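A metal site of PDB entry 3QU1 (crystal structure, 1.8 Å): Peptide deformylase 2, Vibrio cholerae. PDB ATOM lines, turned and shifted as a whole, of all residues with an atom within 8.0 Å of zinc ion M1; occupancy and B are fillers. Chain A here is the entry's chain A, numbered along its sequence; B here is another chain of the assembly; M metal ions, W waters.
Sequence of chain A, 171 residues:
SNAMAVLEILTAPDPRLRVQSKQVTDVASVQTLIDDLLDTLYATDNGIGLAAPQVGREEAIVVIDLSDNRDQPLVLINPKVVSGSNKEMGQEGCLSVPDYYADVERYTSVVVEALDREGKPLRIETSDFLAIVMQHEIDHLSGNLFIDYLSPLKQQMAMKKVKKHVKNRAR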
ATOM      1  N   ILE A   9     -30.408   7.628  28.334  1.00  0.00           N
ATOM      2  CA  ILE A   9     -29.101   8.255  28.349  1.00  0.00           C
ATOM      3  C   ILE A   9     -28.117   7.269  28.942  1.00  0.00           C
ATOM      4  O   ILE A   9     -28.295   6.766  30.071  1.00  0.00           O
ATOM      5  CB  ILE A   9     -29.121   9.545  29.176  1.00  0.00           C
ATOM      6  CG1 ILE A   9     -30.035  10.540  28.496  1.00  0.00           C
ATOM      7  CG2 ILE A   9     -27.695  10.109  29.434  1.00  0.00           C
ATOM      8  CD1 ILE A   9     -30.426  11.723  29.390  1.00  0.00           C
ATOM      9  N   LEU A  17     -20.033   6.083  24.035  1.00  0.00           N
ATOM     10  CA  LEU A  17     -19.692   7.452  24.421  1.00  0.00           C
ATOM     11  C   LEU A  17     -18.362   7.867  23.852  1.00  0.00           C
ATOM     12  O   LEU A  17     -17.994   9.049  23.938  1.00  0.00           O
ATOM     13  CB  LEU A  17     -19.646   7.594  25.953  1.00  0.00           C
ATOM     14  CG  LEU A  17     -20.980   7.404  26.638  1.00  0.00           C
ATOM     15  CD1 LEU A  17     -20.823   7.336  28.150  1.00  0.00           C
ATOM     16  CD2 LEU A  17     -21.950   8.575  26.325  1.00  0.00           C
ATOM     17  N   GLY A  49     -27.887  20.271  28.018  1.00  0.00           N
ATOM     18  CA  GLY A  49     -27.297  19.879  26.740  1.00  0.00           C
ATOM     19  C   GLY A  49     -27.175  18.399  26.587  1.00  0.00           C
ATOM     20  O   GLY A  49     -26.827  17.733  27.523  1.00  0.00           O
ATOM     21  N   LEU A  50     -27.498  17.859  25.416  1.00  0.00           N
ATOM     22  CA  LEU A  50     -27.373  16.428  25.174  1.00  0.00           C
ATOM     23  C   LEU A  50     -26.819  16.229  23.782  1.00  0.00           C
ATOM     24  O   LEU A  50     -27.259  16.882  22.844  1.00  0.00           O
ATOM     25  CB  LEU A  50     -28.725  15.768  25.258  1.00  0.00           C
ATOM     26  CG  LEU A  50     -28.909  14.264  25.177  1.00  0.00           C
ATOM     27  CD1 LEU A  50     -28.242  13.530  26.362  1.00  0.00           C
ATOM     28  CD2 LEU A  50     -30.437  13.895  25.089  1.00  0.00           C
ATOM     29  N   ALA A  51     -25.857  15.336  23.653  1.00  0.00           N
ATOM     30  CA  ALA A  51     -25.249  15.006  22.385  1.00  0.00           C
ATOM     31  C   ALA A  51     -25.645  13.581  21.972  1.00  0.00           C
ATOM     32  O   ALA A  51     -25.799  12.721  22.806  1.00  0.00           O
ATOM     33  CB  ALA A  51     -23.752  15.106  22.556  1.00  0.00           C
ATOM     34  N   GLN A  54     -24.634  10.186  23.531  1.00  0.00           N
ATOM     35  CA  GLN A  54     -25.163   9.892  24.855  1.00  0.00           C
ATOM     36  C   GLN A  54     -26.433   9.078  24.806  1.00  0.00           C
ATOM     37  O   GLN A  54     -26.875   8.530  25.816  1.00  0.00           O
ATOM     38  CB  GLN A  54     -25.390  11.190  25.603  1.00  0.00           C
ATOM     39  CG  GLN A  54     -24.166  12.005  25.776  1.00  0.00           C
ATOM     40  CD  GLN A  54     -24.445  13.243  26.608  1.00  0.00           C
ATOM     41  OE1 GLN A  54     -24.608  14.350  26.051  1.00  0.00           O
ATOM     42  NE2 GLN A  54     -24.539  13.058  27.932  1.00  0.00           N
ATOM     43  N   GLU A  92     -18.246  21.629  35.790  1.00  0.00           N
ATOM     44  CA  GLU A  92     -19.181  20.966  34.910  1.00  0.00           C
ATOM     45  C   GLU A  92     -19.665  19.678  35.504  1.00  0.00           C
ATOM     46  O   GLU A  92     -19.000  19.078  36.366  1.00  0.00           O
ATOM     47  CB  GLU A  92     -18.518  20.618  33.600  1.00  0.00           C
ATOM     48  CG  GLU A  92     -18.252  21.857  32.776  1.00  0.00           C
ATOM     49  CD  GLU A  92     -17.615  21.620  31.414  1.00  0.00           C
ATOM     50  OE1 GLU A  92     -17.835  20.551  30.759  1.00  0.00           O
ATOM     51  OE2 GLU A  92     -16.885  22.564  30.937  1.00  0.00           O
ATOM     52  N   GLY A  93     -20.829  19.244  34.997  1.00  0.00           N
ATOM     53  CA  GLY A  93     -21.293  17.882  35.134  1.00  0.00           C
ATOM     54  C   GLY A  93     -21.666  17.332  33.793  1.00  0.00           C
ATOM     55  O   GLY A  93     -21.400  17.957  32.783  1.00  0.00           O
ATOM     56  N   CYS A  94     -22.253  16.137  33.788  1.00  0.00           N
ATOM     57  CA  CYS A  94     -22.657  15.535  32.539  1.00  0.00           C
ATOM     58  C   CYS A  94     -23.750  14.493  32.794  1.00  0.00           C
ATOM     59  O   CYS A  94     -23.604  13.673  33.667  1.00  0.00           O
ATOM     60  CB  CYS A  94     -21.463  14.892  31.852  1.00  0.00           C
ATOM     61  SG  CYS A  94     -21.814  14.085  30.264  1.00  0.00           S
ATOM     62  N   LEU A  95     -24.799  14.497  31.980  1.00  0.00           N
ATOM     63  CA  LEU A  95     -25.870  13.488  32.102  1.00  0.00           C
ATOM     64  C   LEU A  95     -25.335  12.035  31.971  1.00  0.00           C
ATOM     65  O   LEU A  95     -25.937  11.100  32.533  1.00  0.00           O
ATOM     66  CB  LEU A  95     -26.980  13.801  31.071  1.00  0.00           C
ATOM     67  CG  LEU A  95     -27.684  15.137  31.221  1.00  0.00           C
ATOM     68  CD1 LEU A  95     -28.482  15.427  29.933  1.00  0.00           C
ATOM     69  CD2 LEU A  95     -28.578  15.081  32.452  1.00  0.00           C
ATOM     70  N   SER A  96     -24.216  11.858  31.261  1.00  0.00           N
ATOM     71  CA  SER A  96     -23.631  10.522  31.132  1.00  0.00           C
ATOM     72  C   SER A  96     -22.555  10.186  32.166  1.00  0.00           C
ATOM     73  O   SER A  96     -22.052   9.072  32.153  1.00  0.00           O
ATOM     74  CB  SER A  96     -23.035  10.326  29.736  1.00  0.00           C
ATOM     75  OG  SER A  96     -24.032  10.357  28.746  1.00  0.00           O
ATOM     76  N   VAL A  97     -22.228  11.143  33.051  1.00  0.00           N
ATOM     77  CA  VAL A  97     -21.355  10.932  34.199  1.00  0.00           C
ATOM     78  C   VAL A  97     -22.094  11.470  35.428  1.00  0.00           C
ATOM     79  O   VAL A  97     -21.671  12.447  36.062  1.00  0.00           O
ATOM     80  CB  VAL A  97     -20.020  11.638  34.034  1.00  0.00           C
ATOM     81  CG1 VAL A  97     -19.003  11.162  35.105  1.00  0.00           C
ATOM     82  CG2 VAL A  97     -19.444  11.420  32.641  1.00  0.00           C
ATOM     83  N   ARG A 106     -12.324  25.739  29.858  1.00  0.00           N
ATOM     84  CA  ARG A 106     -12.945  26.020  28.554  1.00  0.00           C
ATOM     85  C   ARG A 106     -12.653  27.461  28.149  1.00  0.00           C
ATOM     86  O   ARG A 106     -12.334  28.271  29.003  1.00  0.00           O
ATOM     87  CB  ARG A 106     -14.453  25.866  28.614  1.00  0.00           C
ATOM     88  CG  ARG A 106     -14.932  24.561  29.165  1.00  0.00           C
ATOM     89  CD  ARG A 106     -14.784  23.439  28.153  1.00  0.00           C
ATOM     90  NE  ARG A 106     -15.453  22.216  28.625  1.00  0.00           N
ATOM     91  CZ  ARG A 106     -15.376  21.032  28.033  1.00  0.00           C
ATOM     92  NH1 ARG A 106     -14.640  20.859  26.942  1.00  0.00           N
ATOM     93  NH2 ARG A 106     -16.039  19.975  28.542  1.00  0.00           N
ATOM     94  N   VAL A 133     -21.319  25.454  27.475  1.00  0.00           N
ATOM     95  CA  VAL A 133     -22.194  24.326  27.164  1.00  0.00           C
ATOM     96  C   VAL A 133     -21.919  23.778  25.753  1.00  0.00           C
ATOM     97  O   VAL A 133     -21.880  22.558  25.498  1.00  0.00           O
ATOM     98  CB  VAL A 133     -23.663  24.758  27.271  1.00  0.00           C
ATOM     99  CG1 VAL A 133     -24.588  23.663  26.752  1.00  0.00           C
ATOM    100  CG2 VAL A 133     -24.046  25.146  28.711  1.00  0.00           C
ATOM    101  N   HIS A 136     -18.700  21.682  25.746  1.00  0.00           N
ATOM    102  CA  HIS A 136     -18.906  20.396  26.429  1.00  0.00           C
ATOM    103  C   HIS A 136     -19.644  19.446  25.481  1.00  0.00           C
ATOM    104  O   HIS A 136     -19.308  18.303  25.344  1.00  0.00           O
ATOM    105  CB  HIS A 136     -19.755  20.648  27.655  1.00  0.00           C
ATOM    106  CG  HIS A 136     -20.204  19.404  28.349  1.00  0.00           C
ATOM    107  ND1 HIS A 136     -19.797  19.075  29.616  1.00  0.00           N
ATOM    108  CD2 HIS A 136     -21.032  18.402  27.946  1.00  0.00           C
ATOM    109  CE1 HIS A 136     -20.347  17.925  29.971  1.00  0.00           C
ATOM    110  NE2 HIS A 136     -21.130  17.521  28.984  1.00  0.00           N
ATOM    111  N   GLU A 137     -20.662  19.941  24.811  1.00  0.00           N
ATOM    112  CA  GLU A 137     -21.504  19.054  24.014  1.00  0.00           C
ATOM    113  C   GLU A 137     -20.830  18.644  22.705  1.00  0.00           C
ATOM    114  O   GLU A 137     -20.895  17.464  22.280  1.00  0.00           O
ATOM    115  CB  GLU A 137     -22.858  19.687  23.731  1.00  0.00           C
ATOM    116  CG  GLU A 137     -23.730  20.031  24.928  1.00  0.00           C
ATOM    117  CD  GLU A 137     -24.017  18.891  25.905  1.00  0.00           C
ATOM    118  OE1 GLU A 137     -24.025  17.739  25.498  1.00  0.00           O
ATOM    119  OE2 GLU A 137     -24.254  19.203  27.104  1.00  0.00           O
ATOM    120  N   ILE A 138     -20.152  19.605  22.068  1.00  0.00           N
ATOM    121  CA  ILE A 138     -19.323  19.311  20.906  1.00  0.00           C
ATOM    122  C   ILE A 138     -18.234  18.266  21.200  1.00  0.00           C
ATOM    123  O   ILE A 138     -17.968  17.371  20.381  1.00  0.00           O
ATOM    124  CB  ILE A 138     -18.773  20.578  20.320  1.00  0.00           C
ATOM    125  CG1 ILE A 138     -19.912  21.438  19.809  1.00  0.00           C
ATOM    126  CG2 ILE A 138     -17.770  20.291  19.185  1.00  0.00           C
ATOM    127  CD1 ILE A 138     -19.451  22.905  19.408  1.00  0.00           C
ATOM    128  N   ASP A 139     -17.626  18.352  22.375  1.00  0.00           N
ATOM    129  CA  ASP A 139     -16.639  17.372  22.851  1.00  0.00           C
ATOM    130  C   ASP A 139     -17.195  15.945  22.790  1.00  0.00           C
ATOM    131  O   ASP A 139     -16.492  15.014  22.455  1.00  0.00           O
ATOM    132  CB  ASP A 139     -16.184  17.691  24.302  1.00  0.00           C
ATOM    133  CG  ASP A 139     -14.759  18.235  24.390  1.00  0.00           C
ATOM    134  OD1 ASP A 139     -14.091  18.421  23.352  1.00  0.00           O
ATOM    135  OD2 ASP A 139     -14.321  18.465  25.525  1.00  0.00           O
ATOM    136  N   HIS A 140     -18.470  15.765  23.121  1.00  0.00           N
ATOM    137  CA  HIS A 140     -19.081  14.411  23.053  1.00  0.00           C
ATOM    138  C   HIS A 140     -18.989  13.798  21.626  1.00  0.00           C
ATOM    139  O   HIS A 140     -18.935  12.585  21.453  1.00  0.00           O
ATOM    140  CB  HIS A 140     -20.564  14.450  23.432  1.00  0.00           C
ATOM    141  CG  HIS A 140     -20.824  14.488  24.897  1.00  0.00           C
ATOM    142  ND1 HIS A 140     -20.421  13.454  25.711  1.00  0.00           N
ATOM    143  CD2 HIS A 140     -21.468  15.379  25.690  1.00  0.00           C
ATOM    144  CE1 HIS A 140     -20.801  13.728  26.951  1.00  0.00           C
ATOM    145  NE2 HIS A 140     -21.496  14.855  26.967  1.00  0.00           N
ATOM    146  N   ASN A 144     -15.321  12.481  23.635  1.00  0.00           N
ATOM    147  CA  ASN A 144     -14.702  12.973  24.825  1.00  0.00           C
ATOM    148  C   ASN A 144     -15.710  13.320  25.934  1.00  0.00           C
ATOM    149  O   ASN A 144     -16.746  13.913  25.678  1.00  0.00           O
ATOM    150  CB  ASN A 144     -13.901  14.240  24.494  1.00  0.00           C
ATOM    151  CG  ASN A 144     -12.758  13.981  23.517  1.00  0.00           C
ATOM    152  OD1 ASN A 144     -12.112  12.955  23.576  1.00  0.00           O
ATOM    153  ND2 ASN A 144     -12.494  14.953  22.639  1.00  0.00           N
ATOM    154  N   LEU A 145     -15.372  12.915  27.171  1.00  0.00           N
ATOM    155  CA  LEU A 145     -16.148  13.289  28.352  1.00  0.00           C
ATOM    156  C   LEU A 145     -15.356  14.300  29.150  1.00  0.00           C
ATOM    157  O   LEU A 145     -14.108  14.295  29.098  1.00  0.00           O
ATOM    158  CB  LEU A 145     -16.397  12.067  29.224  1.00  0.00           C
ATOM    159  CG  LEU A 145     -17.078  10.875  28.514  1.00  0.00           C
ATOM    160  CD1 LEU A 145     -17.290   9.744  29.530  1.00  0.00           C
ATOM    161  CD2 LEU A 145     -18.416  11.326  27.881  1.00  0.00           C
ATOM    162  N   PHE A 146     -16.032  15.164  29.893  1.00  0.00           N
ATOM    163  CA  PHE A 146     -15.289  16.218  30.650  1.00  0.00           C
ATOM    164  C   PHE A 146     -14.255  15.662  31.612  1.00  0.00           C
ATOM    165  O   PHE A 146     -13.187  16.274  31.813  1.00  0.00           O
ATOM    166  CB  PHE A 146     -16.234  17.214  31.346  1.00  0.00           C
ATOM    167  CG  PHE A 146     -16.833  16.704  32.616  1.00  0.00           C
ATOM    168  CD1 PHE A 146     -16.330  17.143  33.825  1.00  0.00           C
ATOM    169  CD2 PHE A 146     -17.916  15.834  32.626  1.00  0.00           C
ATOM    170  CE1 PHE A 146     -16.840  16.684  35.012  1.00  0.00           C
ATOM    171  CE2 PHE A 146     -18.434  15.396  33.813  1.00  0.00           C
ATOM    172  CZ  PHE A 146     -17.904  15.841  35.006  1.00  0.00           C
ATOM    173  N   ALA B 170     -23.756  23.462  33.979  1.00  0.00           N
ATOM    174  CA  ALA B 170     -23.482  22.643  32.757  1.00  0.00           C
ATOM    175  C   ALA B 170     -23.749  21.120  32.992  1.00  0.00           C
ATOM    176  O   ALA B 170     -23.023  20.488  33.733  1.00  0.00           O
ATOM    177  CB  ALA B 170     -22.082  22.875  32.279  1.00  0.00           C
ATOM    178  N   ARG B 171     -24.758  20.567  32.318  1.00  0.00           N
ATOM    179  CA  ARG B 171     -25.004  19.110  32.281  1.00  0.00           C
ATOM    180  C   ARG B 171     -25.371  18.770  30.843  1.00  0.00           C
ATOM    181  O   ARG B 171     -26.363  19.319  30.336  1.00  0.00           O
ATOM    182  CB  ARG B 171     -26.143  18.758  33.199  1.00  0.00           C
ATOM    183  CG  ARG B 171     -25.771  18.738  34.680  1.00  0.00           C
ATOM    184  CD  ARG B 171     -26.961  18.356  35.490  1.00  0.00           C
ATOM    185  NE  ARG B 171     -26.721  18.432  36.919  1.00  0.00           N
ATOM    186  CZ  ARG B 171     -26.751  19.539  37.660  1.00  0.00           C
ATOM    187  NH1 ARG B 171     -26.993  20.769  37.106  1.00  0.00           N
ATOM    188  NH2 ARG B 171     -26.546  19.433  38.968  1.00  0.00           N
ATOM    189  OXT ARG B 171     -24.684  18.017  30.215  1.00  0.00           O
HETATM  190 ZN    ZN M   1     -22.153  15.711  28.690  1.00  0.00          ZN
HETATM  191 ZN    ZN M   2     -24.859  17.827  28.258  1.00  0.00          ZN
HETATM  192  O   HOH W   1     -23.988  16.105  28.117  1.00  0.00           O
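OE1 of Gln 54 sits close to NE2 of His 140 (3.3 Å).
A ring nitrogen (ND1) of His 136 sits at hydrogen-bond distance from the side-chain carboxylate (OE1) of Glu 92 (2.7 Å).
NE2 of Gln 54 lies close to SG of Cys 94 (3.7 Å).
The side-chain sulfur (SG) of Cys 94 sits close to the backbone NH (N) of Ser 96.
OE1 of Gln 54 sits close to OE1 of Glu 137 (3.5 Å).
The side-chain amide nitrogen (NE2) of Gln 54 is in hydrogen-bond range of the side-chain hydroxyl (OG) of Ser 96, 2.9 Å away.
OE1 of Gln 54 is in hydrogen-bond range of N of Ala 51.
Water W1 bridges the side-chain amide oxygen (OE1) of Gln 54 (2.8 Å) and the side-chain carboxylate (OE1) of Glu 137 (3.1 Å).
Gln 54 touches zinc ion M1.
Arg 171 of chain B touches zinc ion M1.
Of the 24 residues printed, 5 come within 4 Å of zinc ion M1.
The nearest printed residue that does not touch zinc ion M1 is Glu 137 (4.2 Å).
Zinc ion M1 is bound by water W1, NE2 of His 140, NE2 of His 136 and SG of Cys 94.
Zinc ion M1 has four donor atoms within binding distance.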
